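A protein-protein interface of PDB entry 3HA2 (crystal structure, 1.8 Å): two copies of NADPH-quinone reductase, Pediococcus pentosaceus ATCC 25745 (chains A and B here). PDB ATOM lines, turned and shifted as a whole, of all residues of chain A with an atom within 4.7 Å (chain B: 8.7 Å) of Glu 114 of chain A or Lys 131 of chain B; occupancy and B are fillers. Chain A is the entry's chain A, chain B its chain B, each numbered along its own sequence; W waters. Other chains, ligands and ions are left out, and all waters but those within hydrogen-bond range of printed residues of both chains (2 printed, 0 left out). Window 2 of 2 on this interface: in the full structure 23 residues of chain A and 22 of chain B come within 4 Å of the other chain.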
ATOM      1  N   TRP A  63       8.586  -5.230  22.550  1.00  0.00           N
ATOM      2  CA  TRP A  63       9.144  -4.108  21.760  1.00  0.00           C
ATOM      3  C   TRP A  63       8.884  -4.240  20.253  1.00  0.00           C
ATOM      4  O   TRP A  63       9.817  -4.193  19.433  1.00  0.00           O
ATOM      5  CB  TRP A  63      10.651  -3.895  22.034  1.00  0.00           C
ATOM      6  CG  TRP A  63      10.929  -3.372  23.434  1.00  0.00           C
ATOM      7  CD1 TRP A  63      11.654  -4.000  24.404  1.00  0.00           C
ATOM      8  CD2 TRP A  63      10.466  -2.139  24.011  1.00  0.00           C
ATOM      9  NE1 TRP A  63      11.674  -3.232  25.546  1.00  0.00           N
ATOM     10  CE2 TRP A  63      10.961  -2.086  25.334  1.00  0.00           C
ATOM     11  CE3 TRP A  63       9.697  -1.067  23.532  1.00  0.00           C
ATOM     12  CZ2 TRP A  63      10.702  -1.002  26.203  1.00  0.00           C
ATOM     13  CZ3 TRP A  63       9.435   0.010  24.394  1.00  0.00           C
ATOM     14  CH2 TRP A  63       9.938   0.032  25.714  1.00  0.00           C
ATOM     15  N   TYR A  64       7.603  -4.402  19.914  1.00  0.00           N
ATOM     16  CA  TYR A  64       7.108  -4.382  18.544  1.00  0.00           C
ATOM     17  C   TYR A  64       7.614  -5.546  17.674  1.00  0.00           C
ATOM     18  O   TYR A  64       7.538  -5.474  16.452  1.00  0.00           O
ATOM     19  CB  TYR A  64       7.413  -3.015  17.895  1.00  0.00           C
ATOM     20  CG  TYR A  64       7.000  -1.883  18.787  1.00  0.00           C
ATOM     21  CD1 TYR A  64       5.664  -1.508  18.885  1.00  0.00           C
ATOM     22  CD2 TYR A  64       7.938  -1.201  19.559  1.00  0.00           C
ATOM     23  CE1 TYR A  64       5.265  -0.477  19.699  1.00  0.00           C
ATOM     24  CE2 TYR A  64       7.550  -0.177  20.403  1.00  0.00           C
ATOM     25  CZ  TYR A  64       6.213   0.184  20.461  1.00  0.00           C
ATOM     26  OH  TYR A  64       5.821   1.201  21.298  1.00  0.00           O
ATOM     27  N   ALA A 107      -4.368   1.419  19.433  1.00  0.00           N
ATOM     28  CA  ALA A 107      -3.112   2.185  19.468  1.00  0.00           C
ATOM     29  C   ALA A 107      -2.266   1.955  18.206  1.00  0.00           C
ATOM     30  O   ALA A 107      -1.400   2.782  17.863  1.00  0.00           O
ATOM     31  CB  ALA A 107      -2.306   1.794  20.703  1.00  0.00           C
ATOM     32  N   PHE A 108      -2.523   0.838  17.520  1.00  0.00           N
ATOM     33  CA  PHE A 108      -1.705   0.404  16.386  1.00  0.00           C
ATOM     34  C   PHE A 108      -2.302   0.860  15.055  1.00  0.00           C
ATOM     35  O   PHE A 108      -2.848   0.069  14.295  1.00  0.00           O
ATOM     36  CB  PHE A 108      -1.518  -1.114  16.397  1.00  0.00           C
ATOM     37  CG  PHE A 108      -0.746  -1.617  17.577  1.00  0.00           C
ATOM     38  CD1 PHE A 108       0.642  -1.556  17.585  1.00  0.00           C
ATOM     39  CD2 PHE A 108      -1.416  -2.145  18.694  1.00  0.00           C
ATOM     40  CE1 PHE A 108       1.371  -2.029  18.688  1.00  0.00           C
ATOM     41  CE2 PHE A 108      -0.695  -2.601  19.816  1.00  0.00           C
ATOM     42  CZ  PHE A 108       0.698  -2.542  19.809  1.00  0.00           C
ATOM     43  N   GLN A 109      -2.163   2.148  14.777  1.00  0.00           N
ATOM     44  CA  GLN A 109      -2.621   2.726  13.512  1.00  0.00           C
ATOM     45  C   GLN A 109      -2.031   4.114  13.398  1.00  0.00           C
ATOM     46  O   GLN A 109      -1.608   4.702  14.404  1.00  0.00           O
ATOM     47  CB  GLN A 109      -4.161   2.840  13.460  1.00  0.00           C
ATOM     48  CG  GLN A 109      -4.772   3.664  14.586  1.00  0.00           C
ATOM     49  CD  GLN A 109      -6.276   3.718  14.545  1.00  0.00           C
ATOM     50  OE1 GLN A 109      -6.873   4.065  13.521  1.00  0.00           O
ATOM     51  NE2 GLN A 109      -6.905   3.432  15.681  1.00  0.00           N
ATOM     52  N   ALA A 112      -2.429   7.315  15.933  1.00  0.00           N
ATOM     53  CA  ALA A 112      -2.606   6.854  17.313  1.00  0.00           C
ATOM     54  C   ALA A 112      -1.255   6.707  17.991  1.00  0.00           C
ATOM     55  O   ALA A 112      -0.225   6.968  17.374  1.00  0.00           O
ATOM     56  CB  ALA A 112      -3.365   5.541  17.351  1.00  0.00           C
ATOM     57  N   ALA A 113      -1.263   6.252  19.246  1.00  0.00           N
ATOM     58  CA  ALA A 113      -0.047   6.221  20.067  1.00  0.00           C
ATOM     59  C   ALA A 113       1.153   5.513  19.407  1.00  0.00           C
ATOM     60  O   ALA A 113       2.287   6.007  19.483  1.00  0.00           O
ATOM     61  CB  ALA A 113      -0.352   5.585  21.436  1.00  0.00           C
ATOM     62  N   GLU A 114       0.902   4.374  18.756  1.00  0.00           N
ATOM     63  CA  GLU A 114       1.974   3.530  18.228  1.00  0.00           C
ATOM     64  C   GLU A 114       2.319   3.780  16.756  1.00  0.00           C
ATOM     65  O   GLU A 114       3.299   3.233  16.254  1.00  0.00           O
ATOM     66  CB  GLU A 114       1.673   2.037  18.472  1.00  0.00           C
ATOM     67  CG  GLU A 114       1.362   1.651  19.922  1.00  0.00           C
ATOM     68  CD  GLU A 114       2.450   2.012  20.946  1.00  0.00           C
ATOM     69  OE1 GLU A 114       3.644   2.154  20.584  1.00  0.00           O
ATOM     70  OE2 GLU A 114       2.094   2.137  22.139  1.00  0.00           O
ATOM     71  N   LYS A 115       1.495   4.591  16.085  1.00  0.00           N
ATOM     72  CA  LYS A 115       1.696   5.059  14.702  1.00  0.00           C
ATOM     73  C   LYS A 115       1.635   3.987  13.617  1.00  0.00           C
ATOM     74  O   LYS A 115       1.331   4.320  12.460  1.00  0.00           O
ATOM     75  CB  LYS A 115       3.007   5.862  14.541  1.00  0.00           C
ATOM     76  CG  LYS A 115       3.134   7.091  15.475  1.00  0.00           C
ATOM     77  CD  LYS A 115       4.367   7.902  15.096  1.00  0.00           C
ATOM     78  CE  LYS A 115       4.305   9.298  15.697  1.00  0.00           C
ATOM     79  NZ  LYS A 115       5.615   9.958  15.476  1.00  0.00           N
ATOM     80  N   PHE A 116       1.944   2.737  13.961  1.00  0.00           N
ATOM     81  CA  PHE A 116       2.025   1.654  12.951  1.00  0.00           C
ATOM     82  C   PHE A 116       1.096   0.503  13.257  1.00  0.00           C
ATOM     83  O   PHE A 116       0.893   0.138  14.420  1.00  0.00           O
ATOM     84  CB  PHE A 116       3.463   1.138  12.815  1.00  0.00           C
ATOM     85  CG  PHE A 116       4.461   2.246  12.656  1.00  0.00           C
ATOM     86  CD1 PHE A 116       4.485   3.012  11.474  1.00  0.00           C
ATOM     87  CD2 PHE A 116       5.346   2.546  13.687  1.00  0.00           C
ATOM     88  CE1 PHE A 116       5.400   4.073  11.338  1.00  0.00           C
ATOM     89  CE2 PHE A 116       6.277   3.585  13.553  1.00  0.00           C
ATOM     90  CZ  PHE A 116       6.293   4.351  12.399  1.00  0.00           C
ATOM     91  N   THR B  80      10.434  -1.709  31.209  1.00  0.00           N
ATOM     92  CA  THR B  80       9.449  -0.643  31.329  1.00  0.00           C
ATOM     93  C   THR B  80       9.951   0.422  32.297  1.00  0.00           C
ATOM     94  O   THR B  80       9.834   1.618  32.027  1.00  0.00           O
ATOM     95  CB  THR B  80       8.077  -1.203  31.781  1.00  0.00           C
ATOM     96  OG1 THR B  80       7.632  -2.139  30.790  1.00  0.00           O
ATOM     97  CG2 THR B  80       7.043  -0.093  31.843  1.00  0.00           C
ATOM     98  N   ALA B  83      13.250   2.348  30.459  1.00  0.00           N
ATOM     99  CA  ALA B  83      13.032   2.940  29.137  1.00  0.00           C
ATOM    100  C   ALA B  83      11.784   3.806  29.049  1.00  0.00           C
ATOM    101  O   ALA B  83      11.726   4.708  28.218  1.00  0.00           O
ATOM    102  CB  ALA B  83      12.986   1.855  28.077  1.00  0.00           C
ATOM    103  N   THR B  84      10.781   3.496  29.872  1.00  0.00           N
ATOM    104  CA  THR B  84       9.533   4.264  29.926  1.00  0.00           C
ATOM    105  C   THR B  84       9.199   4.545  31.374  1.00  0.00           C
ATOM    106  O   THR B  84      10.018   5.131  32.081  1.00  0.00           O
ATOM    107  CB  THR B  84       8.351   3.561  29.173  1.00  0.00           C
ATOM    108  OG1 THR B  84       8.145   2.241  29.713  1.00  0.00           O
ATOM    109  CG2 THR B  84       8.698   3.436  27.689  1.00  0.00           C
ATOM    110  N   GLY B  85       8.026   4.107  31.828  1.00  0.00           N
ATOM    111  CA  GLY B  85       7.633   4.281  33.244  1.00  0.00           C
ATOM    112  C   GLY B  85       7.701   5.731  33.683  1.00  0.00           C
ATOM    113  O   GLY B  85       7.036   6.594  33.105  1.00  0.00           O
ATOM    114  N   TYR B  88      12.123   7.202  31.673  1.00  0.00           N
ATOM    115  CA  TYR B  88      12.400   7.540  30.269  1.00  0.00           C
ATOM    116  C   TYR B  88      13.877   7.881  30.101  1.00  0.00           C
ATOM    117  O   TYR B  88      14.248   8.996  29.696  1.00  0.00           O
ATOM    118  CB  TYR B  88      11.482   8.676  29.774  1.00  0.00           C
ATOM    119  CG  TYR B  88      10.107   8.168  29.402  1.00  0.00           C
ATOM    120  CD1 TYR B  88       9.811   7.814  28.093  1.00  0.00           C
ATOM    121  CD2 TYR B  88       9.115   7.983  30.376  1.00  0.00           C
ATOM    122  CE1 TYR B  88       8.544   7.323  27.735  1.00  0.00           C
ATOM    123  CE2 TYR B  88       7.841   7.493  30.028  1.00  0.00           C
ATOM    124  CZ  TYR B  88       7.575   7.169  28.712  1.00  0.00           C
ATOM    125  OH  TYR B  88       6.341   6.672  28.360  1.00  0.00           O
ATOM    126  N   ALA B  89      14.710   6.899  30.419  1.00  0.00           N
ATOM    127  CA  ALA B  89      16.157   7.107  30.518  1.00  0.00           C
ATOM    128  C   ALA B  89      16.791   7.514  29.203  1.00  0.00           C
ATOM    129  O   ALA B  89      17.841   8.157  29.202  1.00  0.00           O
ATOM    130  CB  ALA B  89      16.842   5.857  31.075  1.00  0.00           C
ATOM    131  N   LEU B  90      16.145   7.163  28.093  1.00  0.00           N
ATOM    132  CA  LEU B  90      16.692   7.385  26.758  1.00  0.00           C
ATOM    133  C   LEU B  90      16.166   8.649  26.087  1.00  0.00           C
ATOM    134  O   LEU B  90      16.567   8.972  24.963  1.00  0.00           O
ATOM    135  CB  LEU B  90      16.403   6.169  25.869  1.00  0.00           C
ATOM    136  CG  LEU B  90      16.815   4.837  26.508  1.00  0.00           C
ATOM    137  CD1 LEU B  90      16.320   3.681  25.695  1.00  0.00           C
ATOM    138  CD2 LEU B  90      18.319   4.782  26.692  1.00  0.00           C
ATOM    139  N   GLU B  91      15.270   9.367  26.764  1.00  0.00           N
ATOM    140  CA  GLU B  91      14.638  10.539  26.164  1.00  0.00           C
ATOM    141  C   GLU B  91      15.688  11.534  25.638  1.00  0.00           C
ATOM    142  O   GLU B  91      16.614  11.927  26.367  1.00  0.00           O
ATOM    143  CB  GLU B  91      13.706  11.256  27.158  1.00  0.00           C
ATOM    144  CG  GLU B  91      13.016  12.482  26.523  1.00  0.00           C
ATOM    145  CD  GLU B  91      11.914  13.085  27.383  1.00  0.00           C
ATOM    146  OE1 GLU B  91      11.745  12.655  28.544  1.00  0.00           O
ATOM    147  OE2 GLU B  91      11.239  14.017  26.887  1.00  0.00           O
ATOM    148  N   ARG B 123      10.953  -0.968  11.067  1.00  0.00           N
ATOM    149  CA  ARG B 123       9.877  -0.283  11.796  1.00  0.00           C
ATOM    150  C   ARG B 123       9.842  -0.588  13.304  1.00  0.00           C
ATOM    151  O   ARG B 123       9.557   0.305  14.094  1.00  0.00           O
ATOM    152  CB  ARG B 123       8.502  -0.583  11.176  1.00  0.00           C
ATOM    153  CG  ARG B 123       7.479   0.510  11.463  1.00  0.00           C
ATOM    154  CD  ARG B 123       7.898   1.795  10.739  1.00  0.00           C
ATOM    155  NE  ARG B 123       7.400   1.789   9.378  1.00  0.00           N
ATOM    156  CZ  ARG B 123       7.800   2.588   8.385  1.00  0.00           C
ATOM    157  NH1 ARG B 123       8.761   3.507   8.538  1.00  0.00           N
ATOM    158  NH2 ARG B 123       7.226   2.442   7.210  1.00  0.00           N
ATOM    159  N   PRO B 124      10.124  -1.845  13.718  1.00  0.00           N
ATOM    160  CA  PRO B 124      10.133  -2.075  15.192  1.00  0.00           C
ATOM    161  C   PRO B 124      11.092  -1.155  15.968  1.00  0.00           C
ATOM    162  O   PRO B 124      10.786  -0.719  17.093  1.00  0.00           O
ATOM    163  CB  PRO B 124      10.562  -3.545  15.304  1.00  0.00           C
ATOM    164  CG  PRO B 124      10.078  -4.163  14.010  1.00  0.00           C
ATOM    165  CD  PRO B 124      10.363  -3.095  12.971  1.00  0.00           C
ATOM    166  N   PHE B 125      12.233  -0.824  15.363  1.00  0.00           N
ATOM    167  CA  PHE B 125      13.181   0.081  15.997  1.00  0.00           C
ATOM    168  C   PHE B 125      12.682   1.512  16.009  1.00  0.00           C
ATOM    169  O   PHE B 125      12.916   2.252  16.946  1.00  0.00           O
ATOM    170  CB  PHE B 125      14.523  -0.006  15.292  1.00  0.00           C
ATOM    171  CG  PHE B 125      15.220  -1.294  15.545  1.00  0.00           C
ATOM    172  CD1 PHE B 125      15.728  -1.577  16.823  1.00  0.00           C
ATOM    173  CD2 PHE B 125      15.327  -2.245  14.543  1.00  0.00           C
ATOM    174  CE1 PHE B 125      16.341  -2.789  17.080  1.00  0.00           C
ATOM    175  CE2 PHE B 125      15.943  -3.468  14.790  1.00  0.00           C
ATOM    176  CZ  PHE B 125      16.462  -3.734  16.045  1.00  0.00           C
ATOM    177  N   GLU B 126      12.018   1.901  14.927  1.00  0.00           N
ATOM    178  CA  GLU B 126      11.432   3.233  14.826  1.00  0.00           C
ATOM    179  C   GLU B 126      10.360   3.390  15.885  1.00  0.00           C
ATOM    180  O   GLU B 126      10.276   4.437  16.564  1.00  0.00           O
ATOM    181  CB  GLU B 126      10.823   3.430  13.431  1.00  0.00           C
ATOM    182  CG  GLU B 126      10.314   4.861  13.179  1.00  0.00           C
ATOM    183  CD  GLU B 126       9.965   5.112  11.717  1.00  0.00           C
ATOM    184  OE1 GLU B 126      10.210   4.206  10.874  1.00  0.00           O
ATOM    185  OE2 GLU B 126       9.435   6.217  11.427  1.00  0.00           O
ATOM    186  N   ALA B 127       9.520   2.366  16.015  1.00  0.00           N
ATOM    187  CA  ALA B 127       8.470   2.346  17.043  1.00  0.00           C
ATOM    188  C   ALA B 127       9.073   2.452  18.436  1.00  0.00           C
ATOM    189  O   ALA B 127       8.548   3.153  19.311  1.00  0.00           O
ATOM    190  CB  ALA B 127       7.623   1.057  16.925  1.00  0.00           C
ATOM    191  N   PHE B 128      10.169   1.737  18.648  1.00  0.00           N
ATOM    192  CA  PHE B 128      10.891   1.832  19.917  1.00  0.00           C
ATOM    193  C   PHE B 128      11.385   3.260  20.198  1.00  0.00           C
ATOM    194  O   PHE B 128      11.188   3.795  21.290  1.00  0.00           O
ATOM    195  CB  PHE B 128      12.072   0.853  19.921  1.00  0.00           C
ATOM    196  CG  PHE B 128      12.938   0.973  21.141  1.00  0.00           C
ATOM    197  CD1 PHE B 128      12.559   0.377  22.333  1.00  0.00           C
ATOM    198  CD2 PHE B 128      14.132   1.696  21.097  1.00  0.00           C
ATOM    199  CE1 PHE B 128      13.357   0.499  23.469  1.00  0.00           C
ATOM    200  CE2 PHE B 128      14.943   1.817  22.242  1.00  0.00           C
ATOM    201  CZ  PHE B 128      14.548   1.230  23.415  1.00  0.00           C
ATOM    202  N   ALA B 129      12.044   3.875  19.219  1.00  0.00           N
ATOM    203  CA  ALA B 129      12.514   5.243  19.390  1.00  0.00           C
ATOM    204  C   ALA B 129      11.360   6.186  19.716  1.00  0.00           C
ATOM    205  O   ALA B 129      11.492   7.032  20.587  1.00  0.00           O
ATOM    206  CB  ALA B 129      13.243   5.707  18.155  1.00  0.00           C
ATOM    207  N   ASN B 130      10.218   6.019  19.051  1.00  0.00           N
ATOM    208  CA  ASN B 130       9.071   6.908  19.313  1.00  0.00           C
ATOM    209  C   ASN B 130       8.585   6.724  20.752  1.00  0.00           C
ATOM    210  O   ASN B 130       8.310   7.703  21.477  1.00  0.00           O
ATOM    211  CB  ASN B 130       7.900   6.660  18.333  1.00  0.00           C
ATOM    212  CG  ASN B 130       8.197   7.096  16.891  1.00  0.00           C
ATOM    213  OD1 ASN B 130       7.595   6.563  15.939  1.00  0.00           O
ATOM    214  ND2 ASN B 130       9.111   8.049  16.716  1.00  0.00           N
ATOM    215  N   LYS B 131       8.489   5.463  21.155  1.00  0.00           N
ATOM    216  CA  LYS B 131       7.960   5.110  22.473  1.00  0.00           C
ATOM    217  C   LYS B 131       8.834   5.659  23.583  1.00  0.00           C
ATOM    218  O   LYS B 131       8.331   6.124  24.620  1.00  0.00           O
ATOM    219  CB  LYS B 131       7.818   3.595  22.618  1.00  0.00           C
ATOM    220  CG  LYS B 131       7.101   3.137  23.904  1.00  0.00           C
ATOM    221  CD  LYS B 131       5.660   3.641  23.878  1.00  0.00           C
ATOM    222  CE  LYS B 131       4.760   2.878  24.808  1.00  0.00           C
ATOM    223  NZ  LYS B 131       3.364   3.341  24.530  1.00  0.00           N
ATOM    224  N   THR B 132      10.139   5.604  23.360  1.00  0.00           N
ATOM    225  CA  THR B 132      11.108   5.977  24.387  1.00  0.00           C
ATOM    226  C   THR B 132      11.575   7.411  24.243  1.00  0.00           C
ATOM    227  O   THR B 132      12.474   7.853  24.975  1.00  0.00           O
ATOM    228  CB  THR B 132      12.320   5.024  24.343  1.00  0.00           C
ATOM    229  OG1 THR B 132      12.896   5.046  23.036  1.00  0.00           O
ATOM    230  CG2 THR B 132      11.873   3.622  24.649  1.00  0.00           C
ATOM    231  N   LYS B 133      10.975   8.123  23.282  1.00  0.00           N
ATOM    232  CA  LYS B 133      11.232   9.554  23.055  1.00  0.00           C
ATOM    233  C   LYS B 133      12.675   9.831  22.602  1.00  0.00           C
ATOM    234  O   LYS B 133      13.254  10.890  22.911  1.00  0.00           O
ATOM    235  CB  LYS B 133      10.895  10.352  24.323  1.00  0.00           C
ATOM    236  CG  LYS B 133       9.424  10.265  24.709  1.00  0.00           C
ATOM    237  CD  LYS B 133       9.125  11.185  25.872  1.00  0.00           C
ATOM    238  CE  LYS B 133       7.792  10.837  26.531  1.00  0.00           C
ATOM    239  NZ  LYS B 133       6.664  10.898  25.564  1.00  0.00           N
ATOM    240  N   MET B 134      13.240   8.876  21.879  1.00  0.00           N
ATOM    241  CA  MET B 134      14.535   9.050  21.248  1.00  0.00           C
ATOM    242  C   MET B 134      14.351   9.700  19.880  1.00  0.00           C
ATOM    243  O   MET B 134      13.236   9.721  19.339  1.00  0.00           O
ATOM    244  CB  MET B 134      15.239   7.698  21.093  1.00  0.00           C
ATOM    245  CG  MET B 134      15.512   6.987  22.408  1.00  0.00           C
ATOM    246  SD  MET B 134      16.421   5.305  22.056  1.00  0.00           S
ATOM    247  CE  MET B 134      18.248   6.028  21.863  1.00  0.00           C
ATOM    248  N   MET B 135      15.436  10.218  19.321  1.00  0.00           N
ATOM    249  CA  MET B 135      15.394  10.864  18.021  1.00  0.00           C
ATOM    250  C   MET B 135      15.971   9.877  16.977  1.00  0.00           C
ATOM    251  O   MET B 135      17.173   9.630  16.947  1.00  0.00           O
ATOM    252  CB  MET B 135      16.166  12.201  18.071  1.00  0.00           C
ATOM    253  CG  MET B 135      16.388  12.819  19.510  1.00  0.00           C
ATOM    254  SD  MET B 135      14.986  13.864  20.476  1.00  0.00           S
ATOM    255  CE  MET B 135      14.807  15.345  19.195  1.00  0.00           C
HETATM  256  O   HOH W   1       5.634   4.486  16.785  1.00  0.00           O
HETATM  257  O   HOH W   2       5.778   3.909  19.434  1.00  0.00           O
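O of Glu 126 of chain B lies close to OD1 of Asn 130 of chain B (3.5 Å). The backbone NH (N) of Glu 114 of chain A is in hydrogen-bond range of the backbone carbonyl oxygen (O) of Ala 107 of chain A. The guanidinium group (NH1) of Arg 123 of chain B lies within salt-bridge range of the side-chain carboxylate (OE1) of Glu 126 of chain B (2.8 Å). The side-chain hydroxyl of Tyr 64 of chain A lies within hydrogen-bond range of the side-chain carboxylate of Glu 114 of chain A, 2.5 Å away. The side-chain hydroxyl (OG1) of Thr 132 of chain B sits at hydrogen-bond distance from the backbone carbonyl oxygen (O) of Phe 128 of chain B.
Hydrophobic or aromatic side chains of chain A within 4 Å of the printed part of chain B: Trp 63, Tyr 64 and Phe 116. Along chain A the printed residues that touch a printed residue of chain B span positions 63 to 116. Hydrophobic or aromatic side chains of chain B within 4 Å of the printed part of chain A: Pro 124, Ala 127 and Phe 128. Among the printed residues, Asp or Glu carboxylates within 4 Å of a Lys or Arg side-chain nitrogen of the other chain: Glu 114 of chain A with Lys 131 of chain B (3.0 Å).
Of the printed residues of chain B, Tyr 64 of chain A touches Pro 124, Ala 127, Phe 128 and Lys 131. No residue of chain B comes within 4 Å of Ala 113 of chain A. Glu 114 of chain A touches just one residue of chain B: Lys 131 (3.0 Å). Printed residues of chain B within 4 Å of Lys 115 of chain A: Asn 130 (3.6 Å). Of the printed residues of chain A, Glu 126 of chain B touches Phe 116 (3.8 Å). Printed residues of chain A within 4 Å of Ala 127 of chain B: Tyr 64 (3.5 Å). Printed residues of chain A within 4 Å of Phe 128 of chain B: Trp 63 (3.4 Å) and Tyr 64 (3.7 Å). Of the printed residues of chain A, Lys 131 of chain B touches Trp 63, Tyr 64 and Glu 114. The nearest residue of chain B that does not touch Glu 114 of chain A is Ala 127 of chain B (4.9 Å). The nearest printed residue of chain A that does not touch Lys 131 of chain B is Ala 113 of chain A (5.3 Å). The nearest printed residue of chain A that does not touch Asn 130 of chain B is Phe 116 of chain A (4.04 Å).
No position is printed for both chains.
The side-chain amino group of Lys 131 of chain B lies within salt-bridge range of the side-chain carboxylate of Glu 114 of chain A (3.0 Å).
Trp 63 of chain A touches Phe 128 of chain B (CE3 to CD1, 3.4 Å). Trp 63 of chain A touches Lys 131 of chain B. Tyr 64 of chain A touches Pro 124 of chain B. Tyr 64 of chain A touches Ala 127 of chain B. N of Phe 128 of chain B touches CE2 of Tyr 64 of chain A (3.7 Å). Lys 131 of chain B touches Tyr 64 of chain A. Lys 115 of chain A touches Asn 130 of chain B (CD to OD1, 3.6 Å). CE1 of Phe 116 of chain A touches CD of Arg 123 of chain B, 3.4 Å away. Phe 116 of chain A touches Glu 126 of chain B (CZ to OE2, 3.8 Å).
Water W1 bridges O of Glu 114 of chain A and OD1 of Asn 130 of chain B. Water W2 lies within hydrogen-bond range of O of Ala 127 of chain B, OE1 of Glu 114 of chain A and OH of Tyr 64 of chain A.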
